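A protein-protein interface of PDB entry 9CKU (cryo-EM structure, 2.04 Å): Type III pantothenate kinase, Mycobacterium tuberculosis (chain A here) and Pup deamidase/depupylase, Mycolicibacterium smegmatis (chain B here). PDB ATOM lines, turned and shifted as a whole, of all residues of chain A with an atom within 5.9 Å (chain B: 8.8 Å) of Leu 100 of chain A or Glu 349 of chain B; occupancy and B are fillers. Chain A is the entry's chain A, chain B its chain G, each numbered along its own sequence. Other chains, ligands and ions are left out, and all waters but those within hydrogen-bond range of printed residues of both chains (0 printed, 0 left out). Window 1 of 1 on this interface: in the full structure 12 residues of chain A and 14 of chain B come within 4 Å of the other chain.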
ATOM      1  N   GLY A  93      18.930 -25.017 -12.432  1.00  0.00           N
ATOM      2  CA  GLY A  93      17.493 -24.900 -12.525  1.00  0.00           C
ATOM      3  C   GLY A  93      16.921 -25.188 -13.892  1.00  0.00           C
ATOM      4  O   GLY A  93      15.764 -24.853 -14.145  1.00  0.00           O
ATOM      5  N   VAL A  94      17.695 -25.807 -14.786  1.00  0.00           N
ATOM      6  CA  VAL A  94      17.219 -26.064 -16.140  1.00  0.00           C
ATOM      7  C   VAL A  94      16.019 -27.012 -16.120  1.00  0.00           C
ATOM      8  O   VAL A  94      15.923 -27.921 -15.287  1.00  0.00           O
ATOM      9  CB  VAL A  94      18.358 -26.634 -17.006  1.00  0.00           C
ATOM     10  CG1 VAL A  94      18.976 -27.881 -16.364  1.00  0.00           C
ATOM     11  CG2 VAL A  94      17.871 -26.944 -18.417  1.00  0.00           C
ATOM     12  N   ARG A  95      15.090 -26.787 -17.048  1.00  0.00           N
ATOM     13  CA  ARG A  95      13.972 -27.698 -17.285  1.00  0.00           C
ATOM     14  C   ARG A  95      14.424 -28.752 -18.289  1.00  0.00           C
ATOM     15  O   ARG A  95      14.540 -28.479 -19.485  1.00  0.00           O
ATOM     16  CB  ARG A  95      12.749 -26.944 -17.791  1.00  0.00           C
ATOM     17  CG  ARG A  95      11.857 -26.377 -16.703  1.00  0.00           C
ATOM     18  CD  ARG A  95      10.489 -26.010 -17.258  1.00  0.00           C
ATOM     19  NE  ARG A  95       9.523 -25.693 -16.214  1.00  0.00           N
ATOM     20  CZ  ARG A  95       9.390 -24.504 -15.645  1.00  0.00           C
ATOM     21  NH1 ARG A  95      10.171 -23.487 -15.970  1.00  0.00           N
ATOM     22  NH2 ARG A  95       8.446 -24.327 -14.727  1.00  0.00           N
ATOM     23  N   ILE A  98      12.717 -33.255 -15.884  1.00  0.00           N
ATOM     24  CA  ILE A  98      12.707 -33.744 -14.508  1.00  0.00           C
ATOM     25  C   ILE A  98      12.138 -32.636 -13.625  1.00  0.00           C
ATOM     26  O   ILE A  98      12.771 -31.579 -13.507  1.00  0.00           O
ATOM     27  CB  ILE A  98      14.114 -34.143 -14.035  1.00  0.00           C
ATOM     28  CG1 ILE A  98      14.667 -35.307 -14.868  1.00  0.00           C
ATOM     29  CG2 ILE A  98      14.093 -34.505 -12.554  1.00  0.00           C
ATOM     30  CD1 ILE A  98      14.073 -36.666 -14.541  1.00  0.00           C
ATOM     31  N   PRO A  99      10.980 -32.829 -12.989  1.00  0.00           N
ATOM     32  CA  PRO A  99      10.487 -31.810 -12.050  1.00  0.00           C
ATOM     33  C   PRO A  99      11.471 -31.599 -10.908  1.00  0.00           C
ATOM     34  O   PRO A  99      12.038 -32.552 -10.372  1.00  0.00           O
ATOM     35  CB  PRO A  99       9.164 -32.395 -11.545  1.00  0.00           C
ATOM     36  CG  PRO A  99       8.821 -33.474 -12.460  1.00  0.00           C
ATOM     37  CD  PRO A  99      10.063 -33.974 -13.083  1.00  0.00           C
ATOM     38  N   LEU A 100      11.669 -30.344 -10.536  1.00  0.00           N
ATOM     39  CA  LEU A 100      12.550 -29.979  -9.431  1.00  0.00           C
ATOM     40  C   LEU A 100      11.665 -29.622  -8.239  1.00  0.00           C
ATOM     41  O   LEU A 100      11.178 -28.498  -8.133  1.00  0.00           O
ATOM     42  CB  LEU A 100      13.455 -28.830  -9.825  1.00  0.00           C
ATOM     43  CG  LEU A 100      14.426 -29.149 -10.967  1.00  0.00           C
ATOM     44  CD1 LEU A 100      15.195 -27.897 -11.364  1.00  0.00           C
ATOM     45  CD2 LEU A 100      15.354 -30.326 -10.689  1.00  0.00           C
ATOM     46  N   LEU A 101      11.449 -30.586  -7.345  1.00  0.00           N
ATOM     47  CA  LEU A 101      10.553 -30.398  -6.201  1.00  0.00           C
ATOM     48  C   LEU A 101      11.332 -29.880  -4.990  1.00  0.00           C
ATOM     49  O   LEU A 101      11.438 -30.524  -3.950  1.00  0.00           O
ATOM     50  CB  LEU A 101       9.830 -31.696  -5.878  1.00  0.00           C
ATOM     51  CG  LEU A 101       9.058 -32.333  -7.033  1.00  0.00           C
ATOM     52  CD1 LEU A 101       8.221 -33.495  -6.534  1.00  0.00           C
ATOM     53  CD2 LEU A 101       8.191 -31.307  -7.770  1.00  0.00           C
ATOM     54  N   VAL A 102      11.879 -28.679  -5.148  1.00  0.00           N
ATOM     55  CA  VAL A 102      12.655 -28.018  -4.110  1.00  0.00           C
ATOM     56  C   VAL A 102      12.177 -26.574  -3.982  1.00  0.00           C
ATOM     57  O   VAL A 102      11.358 -26.095  -4.763  1.00  0.00           O
ATOM     58  CB  VAL A 102      14.171 -28.069  -4.393  1.00  0.00           C
ATOM     59  CG1 VAL A 102      14.660 -29.514  -4.437  1.00  0.00           C
ATOM     60  CG2 VAL A 102      14.499 -27.337  -5.690  1.00  0.00           C
ATOM     61  N   PRO A 105      14.428 -23.811  -7.416  1.00  0.00           N
ATOM     62  CA  PRO A 105      15.083 -24.643  -8.442  1.00  0.00           C
ATOM     63  C   PRO A 105      16.332 -24.015  -9.033  1.00  0.00           C
ATOM     64  O   PRO A 105      17.237 -24.737  -9.459  1.00  0.00           O
ATOM     65  CB  PRO A 105      13.987 -24.810  -9.501  1.00  0.00           C
ATOM     66  CG  PRO A 105      12.718 -24.655  -8.754  1.00  0.00           C
ATOM     67  CD  PRO A 105      12.987 -23.659  -7.671  1.00  0.00           C
ATOM     68  N   LYS A 106      16.414 -22.686  -9.042  1.00  0.00           N
ATOM     69  CA  LYS A 106      17.551 -22.001  -9.637  1.00  0.00           C
ATOM     70  C   LYS A 106      18.859 -22.283  -8.911  1.00  0.00           C
ATOM     71  O   LYS A 106      19.922 -22.058  -9.491  1.00  0.00           O
ATOM     72  CB  LYS A 106      17.283 -20.499  -9.652  1.00  0.00           C
ATOM     73  CG  LYS A 106      16.214 -20.088 -10.646  1.00  0.00           C
ATOM     74  CD  LYS A 106      16.284 -18.612 -10.982  1.00  0.00           C
ATOM     75  CE  LYS A 106      17.278 -18.346 -12.087  1.00  0.00           C
ATOM     76  NZ  LYS A 106      16.797 -18.860 -13.400  1.00  0.00           N
ATOM     77  N   VAL A 108      19.701 -25.333  -7.847  1.00  0.00           N
ATOM     78  CA  VAL A 108      20.060 -26.725  -8.089  1.00  0.00           C
ATOM     79  C   VAL A 108      21.048 -26.763  -9.250  1.00  0.00           C
ATOM     80  O   VAL A 108      20.715 -26.376 -10.375  1.00  0.00           O
ATOM     81  CB  VAL A 108      18.818 -27.583  -8.379  1.00  0.00           C
ATOM     82  CG1 VAL A 108      19.192 -29.049  -8.533  1.00  0.00           C
ATOM     83  CG2 VAL A 108      17.792 -27.417  -7.274  1.00  0.00           C
ATOM     84  N   ILE A 113      21.028 -32.196 -11.675  1.00  0.00           N
ATOM     85  CA  ILE A 113      19.869 -32.408 -12.536  1.00  0.00           C
ATOM     86  C   ILE A 113      20.193 -33.424 -13.622  1.00  0.00           C
ATOM     87  O   ILE A 113      19.423 -34.353 -13.874  1.00  0.00           O
ATOM     88  CB  ILE A 113      19.404 -31.077 -13.155  1.00  0.00           C
ATOM     89  CG1 ILE A 113      18.945 -30.093 -12.077  1.00  0.00           C
ATOM     90  CG2 ILE A 113      18.288 -31.330 -14.160  1.00  0.00           C
ATOM     91  CD1 ILE A 113      18.953 -28.661 -12.538  1.00  0.00           C
ATOM     92  N   PHE A 147      12.701 -34.970  -9.004  1.00  0.00           N
ATOM     93  CA  PHE A 147      13.872 -34.676  -8.186  1.00  0.00           C
ATOM     94  C   PHE A 147      13.416 -34.142  -6.833  1.00  0.00           C
ATOM     95  O   PHE A 147      12.750 -33.103  -6.757  1.00  0.00           O
ATOM     96  CB  PHE A 147      14.782 -33.671  -8.886  1.00  0.00           C
ATOM     97  CG  PHE A 147      15.926 -33.199  -8.041  1.00  0.00           C
ATOM     98  CD1 PHE A 147      17.060 -33.980  -7.889  1.00  0.00           C
ATOM     99  CD2 PHE A 147      15.871 -31.977  -7.398  1.00  0.00           C
ATOM    100  CE1 PHE A 147      18.117 -33.546  -7.111  1.00  0.00           C
ATOM    101  CE2 PHE A 147      16.922 -31.537  -6.622  1.00  0.00           C
ATOM    102  CZ  PHE A 147      18.045 -32.321  -6.476  1.00  0.00           C
ATOM    103  N   VAL B 183      -0.151 -18.664  -9.953  1.00  0.00           N
ATOM    104  CA  VAL B 183       0.532 -19.550 -10.894  1.00  0.00           C
ATOM    105  C   VAL B 183      -0.423 -20.620 -11.397  1.00  0.00           C
ATOM    106  O   VAL B 183      -0.261 -21.129 -12.506  1.00  0.00           O
ATOM    107  CB  VAL B 183       1.801 -20.182 -10.275  1.00  0.00           C
ATOM    108  CG1 VAL B 183       2.762 -19.113  -9.830  1.00  0.00           C
ATOM    109  CG2 VAL B 183       1.459 -21.140  -9.139  1.00  0.00           C
ATOM    110  N   SER B 295       7.950 -18.005 -16.351  1.00  0.00           N
ATOM    111  CA  SER B 295       8.731 -19.233 -16.261  1.00  0.00           C
ATOM    112  C   SER B 295       8.533 -19.960 -14.936  1.00  0.00           C
ATOM    113  O   SER B 295       8.920 -21.126 -14.833  1.00  0.00           O
ATOM    114  CB  SER B 295      10.217 -18.941 -16.458  1.00  0.00           C
ATOM    115  OG  SER B 295      10.752 -18.205 -15.377  1.00  0.00           O
ATOM    116  N   LEU B 296       7.951 -19.306 -13.931  1.00  0.00           N
ATOM    117  CA  LEU B 296       7.626 -19.898 -12.636  1.00  0.00           C
ATOM    118  C   LEU B 296       8.866 -20.264 -11.828  1.00  0.00           C
ATOM    119  O   LEU B 296       8.802 -21.130 -10.957  1.00  0.00           O
ATOM    120  CB  LEU B 296       6.727 -21.129 -12.801  1.00  0.00           C
ATOM    121  CG  LEU B 296       5.545 -21.008 -13.766  1.00  0.00           C
ATOM    122  CD1 LEU B 296       4.700 -22.268 -13.737  1.00  0.00           C
ATOM    123  CD2 LEU B 296       4.692 -19.788 -13.452  1.00  0.00           C
ATOM    124  N   ARG B 297       9.995 -19.616 -12.103  1.00  0.00           N
ATOM    125  CA  ARG B 297      11.230 -19.836 -11.368  1.00  0.00           C
ATOM    126  C   ARG B 297      11.544 -18.732 -10.366  1.00  0.00           C
ATOM    127  O   ARG B 297      12.516 -18.859  -9.619  1.00  0.00           O
ATOM    128  CB  ARG B 297      12.402 -19.979 -12.350  1.00  0.00           C
ATOM    129  CG  ARG B 297      12.470 -21.329 -13.054  1.00  0.00           C
ATOM    130  CD  ARG B 297      12.975 -22.408 -12.120  1.00  0.00           C
ATOM    131  NE  ARG B 297      13.361 -23.641 -12.802  1.00  0.00           N
ATOM    132  CZ  ARG B 297      12.620 -24.740 -12.884  1.00  0.00           C
ATOM    133  NH1 ARG B 297      11.391 -24.790 -12.400  1.00  0.00           N
ATOM    134  NH2 ARG B 297      13.136 -25.826 -13.451  1.00  0.00           N
ATOM    135  N   THR B 309       9.610 -20.484  -4.549  1.00  0.00           N
ATOM    136  CA  THR B 309       8.754 -20.186  -5.686  1.00  0.00           C
ATOM    137  C   THR B 309       7.294 -20.303  -5.274  1.00  0.00           C
ATOM    138  O   THR B 309       6.960 -20.832  -4.212  1.00  0.00           O
ATOM    139  CB  THR B 309       9.012 -21.141  -6.855  1.00  0.00           C
ATOM    140  OG1 THR B 309       8.561 -22.456  -6.512  1.00  0.00           O
ATOM    141  CG2 THR B 309      10.484 -21.185  -7.225  1.00  0.00           C
ATOM    142  N   ALA B 310       6.414 -19.804  -6.142  1.00  0.00           N
ATOM    143  CA  ALA B 310       4.988 -19.964  -5.906  1.00  0.00           C
ATOM    144  C   ALA B 310       4.578 -21.430  -5.994  1.00  0.00           C
ATOM    145  O   ALA B 310       3.713 -21.884  -5.241  1.00  0.00           O
ATOM    146  CB  ALA B 310       4.200 -19.110  -6.896  1.00  0.00           C
ATOM    147  N   LEU B 311       5.196 -22.187  -6.902  1.00  0.00           N
ATOM    148  CA  LEU B 311       4.904 -23.614  -6.996  1.00  0.00           C
ATOM    149  C   LEU B 311       5.259 -24.339  -5.698  1.00  0.00           C
ATOM    150  O   LEU B 311       4.511 -25.207  -5.242  1.00  0.00           O
ATOM    151  CB  LEU B 311       5.645 -24.230  -8.187  1.00  0.00           C
ATOM    152  CG  LEU B 311       5.023 -24.046  -9.581  1.00  0.00           C
ATOM    153  CD1 LEU B 311       5.946 -24.582 -10.652  1.00  0.00           C
ATOM    154  CD2 LEU B 311       3.667 -24.716  -9.686  1.00  0.00           C
ATOM    155  N   ALA B 312       6.382 -23.983  -5.077  1.00  0.00           N
ATOM    156  CA  ALA B 312       6.750 -24.598  -3.801  1.00  0.00           C
ATOM    157  C   ALA B 312       5.720 -24.292  -2.713  1.00  0.00           C
ATOM    158  O   ALA B 312       5.319 -25.186  -1.955  1.00  0.00           O
ATOM    159  CB  ALA B 312       8.136 -24.121  -3.382  1.00  0.00           C
ATOM    160  N   ARG B 315       2.720 -26.396  -3.349  1.00  0.00           N
ATOM    161  CA  ARG B 315       2.962 -27.779  -2.942  1.00  0.00           C
ATOM    162  C   ARG B 315       2.834 -27.949  -1.432  1.00  0.00           C
ATOM    163  O   ARG B 315       2.253 -28.933  -0.967  1.00  0.00           O
ATOM    164  CB  ARG B 315       4.341 -28.239  -3.405  1.00  0.00           C
ATOM    165  CG  ARG B 315       4.401 -28.696  -4.843  1.00  0.00           C
ATOM    166  CD  ARG B 315       5.738 -29.339  -5.171  1.00  0.00           C
ATOM    167  NE  ARG B 315       6.493 -28.545  -6.132  1.00  0.00           N
ATOM    168  CZ  ARG B 315       7.543 -27.788  -5.855  1.00  0.00           C
ATOM    169  NH1 ARG B 315       8.051 -27.714  -4.640  1.00  0.00           N
ATOM    170  NH2 ARG B 315       8.107 -27.091  -6.832  1.00  0.00           N
ATOM    171  N   ALA B 342      -2.831 -31.418  -7.650  1.00  0.00           N
ATOM    172  CA  ALA B 342      -1.535 -32.083  -7.736  1.00  0.00           C
ATOM    173  C   ALA B 342      -1.108 -32.280  -9.183  1.00  0.00           C
ATOM    174  O   ALA B 342       0.051 -32.034  -9.528  1.00  0.00           O
ATOM    175  CB  ALA B 342      -1.594 -33.424  -7.009  1.00  0.00           C
ATOM    176  N   ASN B 343      -2.034 -32.702 -10.047  1.00  0.00           N
ATOM    177  CA  ASN B 343      -1.689 -32.894 -11.451  1.00  0.00           C
ATOM    178  C   ASN B 343      -1.242 -31.591 -12.091  1.00  0.00           C
ATOM    179  O   ASN B 343      -0.237 -31.556 -12.808  1.00  0.00           O
ATOM    180  CB  ASN B 343      -2.878 -33.474 -12.214  1.00  0.00           C
ATOM    181  CG  ASN B 343      -2.590 -33.639 -13.696  1.00  0.00           C
ATOM    182  OD1 ASN B 343      -3.285 -33.085 -14.543  1.00  0.00           O
ATOM    183  ND2 ASN B 343      -1.545 -34.390 -14.010  1.00  0.00           N
ATOM    184  N   VAL B 344      -1.973 -30.506 -11.835  1.00  0.00           N
ATOM    185  CA  VAL B 344      -1.615 -29.217 -12.412  1.00  0.00           C
ATOM    186  C   VAL B 344      -0.257 -28.760 -11.901  1.00  0.00           C
ATOM    187  O   VAL B 344       0.563 -28.247 -12.664  1.00  0.00           O
ATOM    188  CB  VAL B 344      -2.720 -28.181 -12.128  1.00  0.00           C
ATOM    189  CG1 VAL B 344      -2.158 -26.769 -12.116  1.00  0.00           C
ATOM    190  CG2 VAL B 344      -3.813 -28.307 -13.167  1.00  0.00           C
ATOM    191  N   LEU B 345      -0.005 -28.906 -10.603  1.00  0.00           N
ATOM    192  CA  LEU B 345       1.290 -28.493 -10.074  1.00  0.00           C
ATOM    193  C   LEU B 345       2.420 -29.297 -10.706  1.00  0.00           C
ATOM    194  O   LEU B 345       3.445 -28.731 -11.108  1.00  0.00           O
ATOM    195  CB  LEU B 345       1.309 -28.623  -8.551  1.00  0.00           C
ATOM    196  CG  LEU B 345       0.380 -27.700  -7.750  1.00  0.00           C
ATOM    197  CD1 LEU B 345       0.656 -27.834  -6.264  1.00  0.00           C
ATOM    198  CD2 LEU B 345       0.501 -26.249  -8.198  1.00  0.00           C
ATOM    199  N   ASP B 346       2.230 -30.610 -10.847  1.00  0.00           N
ATOM    200  CA  ASP B 346       3.239 -31.441 -11.495  1.00  0.00           C
ATOM    201  C   ASP B 346       3.489 -30.980 -12.927  1.00  0.00           C
ATOM    202  O   ASP B 346       4.640 -30.794 -13.341  1.00  0.00           O
ATOM    203  CB  ASP B 346       2.795 -32.905 -11.457  1.00  0.00           C
ATOM    204  CG  ASP B 346       3.680 -33.817 -12.293  1.00  0.00           C
ATOM    205  OD1 ASP B 346       4.910 -33.817 -12.091  1.00  0.00           O
ATOM    206  OD2 ASP B 346       3.137 -34.542 -13.148  1.00  0.00           O
ATOM    207  N   LEU B 347       2.414 -30.751 -13.689  1.00  0.00           N
ATOM    208  CA  LEU B 347       2.565 -30.359 -15.085  1.00  0.00           C
ATOM    209  C   LEU B 347       3.239 -29.001 -15.219  1.00  0.00           C
ATOM    210  O   LEU B 347       4.105 -28.818 -16.080  1.00  0.00           O
ATOM    211  CB  LEU B 347       1.210 -30.345 -15.782  1.00  0.00           C
ATOM    212  CG  LEU B 347       0.514 -31.692 -15.992  1.00  0.00           C
ATOM    213  CD1 LEU B 347      -0.786 -31.481 -16.736  1.00  0.00           C
ATOM    214  CD2 LEU B 347       1.404 -32.682 -16.731  1.00  0.00           C
ATOM    215  N   LEU B 348       2.850 -28.032 -14.385  1.00  0.00           N
ATOM    216  CA  LEU B 348       3.471 -26.714 -14.448  1.00  0.00           C
ATOM    217  C   LEU B 348       4.952 -26.797 -14.126  1.00  0.00           C
ATOM    218  O   LEU B 348       5.766 -26.128 -14.766  1.00  0.00           O
ATOM    219  CB  LEU B 348       2.779 -25.736 -13.495  1.00  0.00           C
ATOM    220  CG  LEU B 348       1.390 -25.214 -13.877  1.00  0.00           C
ATOM    221  CD1 LEU B 348       0.836 -24.336 -12.777  1.00  0.00           C
ATOM    222  CD2 LEU B 348       1.425 -24.452 -15.195  1.00  0.00           C
ATOM    223  N   GLU B 349       5.323 -27.597 -13.124  1.00  0.00           N
ATOM    224  CA  GLU B 349       6.742 -27.753 -12.829  1.00  0.00           C
ATOM    225  C   GLU B 349       7.482 -28.374 -14.010  1.00  0.00           C
ATOM    226  O   GLU B 349       8.573 -27.922 -14.368  1.00  0.00           O
ATOM    227  CB  GLU B 349       6.938 -28.583 -11.565  1.00  0.00           C
ATOM    228  CG  GLU B 349       8.400 -28.891 -11.244  1.00  0.00           C
ATOM    229  CD  GLU B 349       9.292 -27.668 -11.274  1.00  0.00           C
ATOM    230  OE1 GLU B 349       8.871 -26.617 -10.752  1.00  0.00           O
ATOM    231  OE2 GLU B 349      10.410 -27.752 -11.831  1.00  0.00           O
ATOM    232  N   ARG B 350       6.895 -29.393 -14.645  1.00  0.00           N
ATOM    233  CA  ARG B 350       7.565 -30.032 -15.777  1.00  0.00           C
ATOM    234  C   ARG B 350       7.754 -29.055 -16.931  1.00  0.00           C
ATOM    235  O   ARG B 350       8.869 -28.872 -17.429  1.00  0.00           O
ATOM    236  CB  ARG B 350       6.770 -31.259 -16.226  1.00  0.00           C
ATOM    237  CG  ARG B 350       6.898 -32.419 -15.275  1.00  0.00           C
ATOM    238  CD  ARG B 350       6.074 -33.622 -15.669  1.00  0.00           C
ATOM    239  NE  ARG B 350       6.148 -34.674 -14.660  1.00  0.00           N
ATOM    240  CZ  ARG B 350       7.125 -35.567 -14.560  1.00  0.00           C
ATOM    241  NH1 ARG B 350       8.142 -35.584 -15.406  1.00  0.00           N
ATOM    242  NH2 ARG B 350       7.080 -36.470 -13.586  1.00  0.00           N
ATOM    243  N   ASP B 351       6.678 -28.414 -17.364  1.00  0.00           N
ATOM    244  CA  ASP B 351       6.763 -27.375 -18.377  1.00  0.00           C
ATOM    245  C   ASP B 351       5.431 -26.634 -18.437  1.00  0.00           C
ATOM    246  O   ASP B 351       4.385 -27.281 -18.541  1.00  0.00           O
ATOM    247  CB  ASP B 351       7.111 -27.976 -19.739  1.00  0.00           C
ATOM    248  CG  ASP B 351       7.078 -26.955 -20.850  1.00  0.00           C
ATOM    249  OD1 ASP B 351       7.877 -25.994 -20.806  1.00  0.00           O
ATOM    250  OD2 ASP B 351       6.249 -27.110 -21.765  1.00  0.00           O
ATOM    251  N   PRO B 352       5.414 -25.298 -18.373  1.00  0.00           N
ATOM    252  CA  PRO B 352       4.115 -24.596 -18.377  1.00  0.00           C
ATOM    253  C   PRO B 352       3.227 -24.924 -19.568  1.00  0.00           C
ATOM    254  O   PRO B 352       2.006 -25.017 -19.405  1.00  0.00           O
ATOM    255  CB  PRO B 352       4.524 -23.118 -18.362  1.00  0.00           C
ATOM    256  CG  PRO B 352       5.832 -23.104 -17.676  1.00  0.00           C
ATOM    257  CD  PRO B 352       6.524 -24.378 -18.063  1.00  0.00           C
ATOM    258  N   MET B 353       3.795 -25.110 -20.760  1.00  0.00           N
ATOM    259  CA  MET B 353       2.979 -25.339 -21.945  1.00  0.00           C
ATOM    260  C   MET B 353       2.237 -26.666 -21.910  1.00  0.00           C
ATOM    261  O   MET B 353       1.352 -26.877 -22.742  1.00  0.00           O
ATOM    262  CB  MET B 353       3.842 -25.266 -23.204  1.00  0.00           C
ATOM    263  CG  MET B 353       4.354 -23.872 -23.533  1.00  0.00           C
ATOM    264  SD  MET B 353       3.133 -22.796 -24.330  1.00  0.00           S
ATOM    265  CE  MET B 353       2.210 -22.149 -22.940  1.00  0.00           C
ATOM    266  N   GLU B 354       2.562 -27.558 -20.976  1.00  0.00           N
ATOM    267  CA  GLU B 354       1.771 -28.768 -20.792  1.00  0.00           C
ATOM    268  C   GLU B 354       0.418 -28.489 -20.155  1.00  0.00           C
ATOM    269  O   GLU B 354      -0.398 -29.410 -20.050  1.00  0.00           O
ATOM    270  CB  GLU B 354       2.546 -29.782 -19.949  1.00  0.00           C
ATOM    271  CG  GLU B 354       3.815 -30.281 -20.623  1.00  0.00           C
ATOM    272  CD  GLU B 354       4.443 -31.459 -19.910  1.00  0.00           C
ATOM    273  OE1 GLU B 354       3.870 -31.932 -18.905  1.00  0.00           O
ATOM    274  OE2 GLU B 354       5.516 -31.915 -20.355  1.00  0.00           O
ATOM    275  N   CYS B 355       0.170 -27.260 -19.703  1.00  0.00           N
ATOM    276  CA  CYS B 355      -1.147 -26.843 -19.243  1.00  0.00           C
ATOM    277  C   CYS B 355      -1.835 -25.912 -20.233  1.00  0.00           C
ATOM    278  O   CYS B 355      -2.836 -25.283 -19.880  1.00  0.00           O
ATOM    279  CB  CYS B 355      -1.041 -26.164 -17.877  1.00  0.00           C
ATOM    280  SG  CYS B 355      -0.562 -27.260 -16.542  1.00  0.00           S
ATOM    281  N   TRP B 361      -3.852 -18.988 -18.374  1.00  0.00           N
ATOM    282  CA  TRP B 361      -2.708 -18.174 -18.769  1.00  0.00           C
ATOM    283  C   TRP B 361      -1.756 -18.976 -19.653  1.00  0.00           C
ATOM    284  O   TRP B 361      -1.171 -18.387 -20.563  1.00  0.00           O
ATOM    285  CB  TRP B 361      -1.977 -17.545 -17.565  1.00  0.00           C
ATOM    286  CG  TRP B 361      -1.191 -18.468 -16.674  1.00  0.00           C
ATOM    287  CD1 TRP B 361      -1.603 -19.003 -15.490  1.00  0.00           C
ATOM    288  CD2 TRP B 361       0.135 -18.959 -16.892  1.00  0.00           C
ATOM    289  NE1 TRP B 361      -0.625 -19.802 -14.963  1.00  0.00           N
ATOM    290  CE2 TRP B 361       0.456 -19.789 -15.800  1.00  0.00           C
ATOM    291  CE3 TRP B 361       1.082 -18.779 -17.901  1.00  0.00           C
ATOM    292  CZ2 TRP B 361       1.675 -20.440 -15.693  1.00  0.00           C
ATOM    293  CZ3 TRP B 361       2.296 -19.421 -17.788  1.00  0.00           C
ATOM    294  CH2 TRP B 361       2.582 -20.240 -16.693  1.00  0.00           C
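CG of Arg 95 of chain A touches NH2 of Arg 297 of chain B, 3.5 Å away. Arg 95 of chain A touches Asp 351 of chain B. OD1 of Asp 346 of chain B touches CG of Pro 99 of chain A (3.9 Å). CG of Glu 349 of chain B touches CB of Pro 99 of chain A (3.6 Å). Pro 99 of chain A touches Arg 350 of chain B. Leu 100 of chain A touches Arg 297 of chain B. Arg 315 of chain B touches Leu 100 of chain A. Arg 315 of chain B touches Leu 101 of chain A. Pro 105 of chain A touches Arg 297 of chain B. Thr 309 of chain B touches Pro 105 of chain A.
The backbone carbonyl oxygen (O) of Pro 105 of chain A sits close to the backbone NH (N) of Gly 93 of chain A (3.4 Å). The backbone carbonyl oxygen of Val 108 of chain A sits at hydrogen-bond distance from the backbone NH of Gly 93 of chain A (3.0 Å). The backbone NH (N) of Phe 147 of chain A sits at hydrogen-bond distance from the backbone carbonyl oxygen (O) of Pro 99 of chain A (2.9 Å). The side-chain hydroxyl of Thr 309 of chain B sits close to the backbone NH of Leu 311 of chain B, 3.4 Å away. The guanidinium group of Arg 350 of chain B lies within salt-bridge range of the side-chain carboxylate of Asp 346 of chain B (3.0 Å). OD2 of Asp 351 of chain B lies close to N of Met 353 of chain B.
Printed residues of chain B within 4 Å of Arg 95 of chain A: Ser 295 (2.9 Å), Arg 297 (3.5 Å), Leu 348 (3.2 Å), Glu 349 (3.0 Å), Arg 350 (3.3 Å), Asp 351 (3.9 Å) and Pro 352 (3.8 Å). Of the printed residues of chain A, Ser 295 of chain B touches Arg 95 (2.9 Å). Printed residues of chain A within 4 Å of Asp 346 of chain B: Pro 99 (3.9 Å). Of chain A, only Arg 95, Pro 99 and Leu 100 come within 4 Å of Glu 349 of chain B. The nearest residue of chain A that does not touch Glu 349 of chain B is Leu 101 of chain A (4.2 Å).
O of Gly 93 of chain A is in hydrogen-bond range of NH2 of Arg 297 of chain B (2.9 Å). The guanidinium group (NH1) of Arg 95 of chain A is in hydrogen-bond range of the backbone carbonyl oxygen (O) of Ser 295 of chain B (2.9 Å). The guanidinium group (NH2) of Arg 95 of chain A lies within hydrogen-bond range of the backbone carbonyl oxygen (O) of Leu 348 of chain B (3.2 Å). The guanidinium group (NE) of Arg 95 of chain A lies within hydrogen-bond range of the backbone carbonyl oxygen (O) of Glu 349 of chain B, at 3.0 Å. The guanidinium group of Arg 95 of chain A sits close to the backbone carbonyl oxygen of Arg 350 of chain B (3.5 Å). The backbone NH (N) of Leu 100 of chain A is in hydrogen-bond range of the side-chain carboxylate (OE2) of Glu 349 of chain B, at 3.2 Å.
Of the 13 printed residues of chain A, 8 touch a printed residue of chain B. Printed residues of chain A that touch a printed residue of chain B: Gly 93, Val 94, Arg 95, Pro 99, Leu 100, Leu 101, Val 102 and Pro 105. Hydrophobic or aromatic side chains of chain A within 4 Å of the printed part of chain B: Pro 99, Leu 100, Leu 101 and Pro 105. Of the 24 printed residues of chain B, 10 touch a printed residue of chain A. Printed residues of chain B that touch a printed residue of chain A: Ser 295, Arg 297, Thr 309, Arg 315, Asp 346, Leu 348, Glu 349, Arg 350, Asp 351 and Pro 352. Along chain B the printed residues that touch a printed residue of chain A span positions 295 to 352. Among the printed residues, no Asp or Glu carboxylate lies within 4 Å of a Lys or Arg side-chain nitrogen of the other chain.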
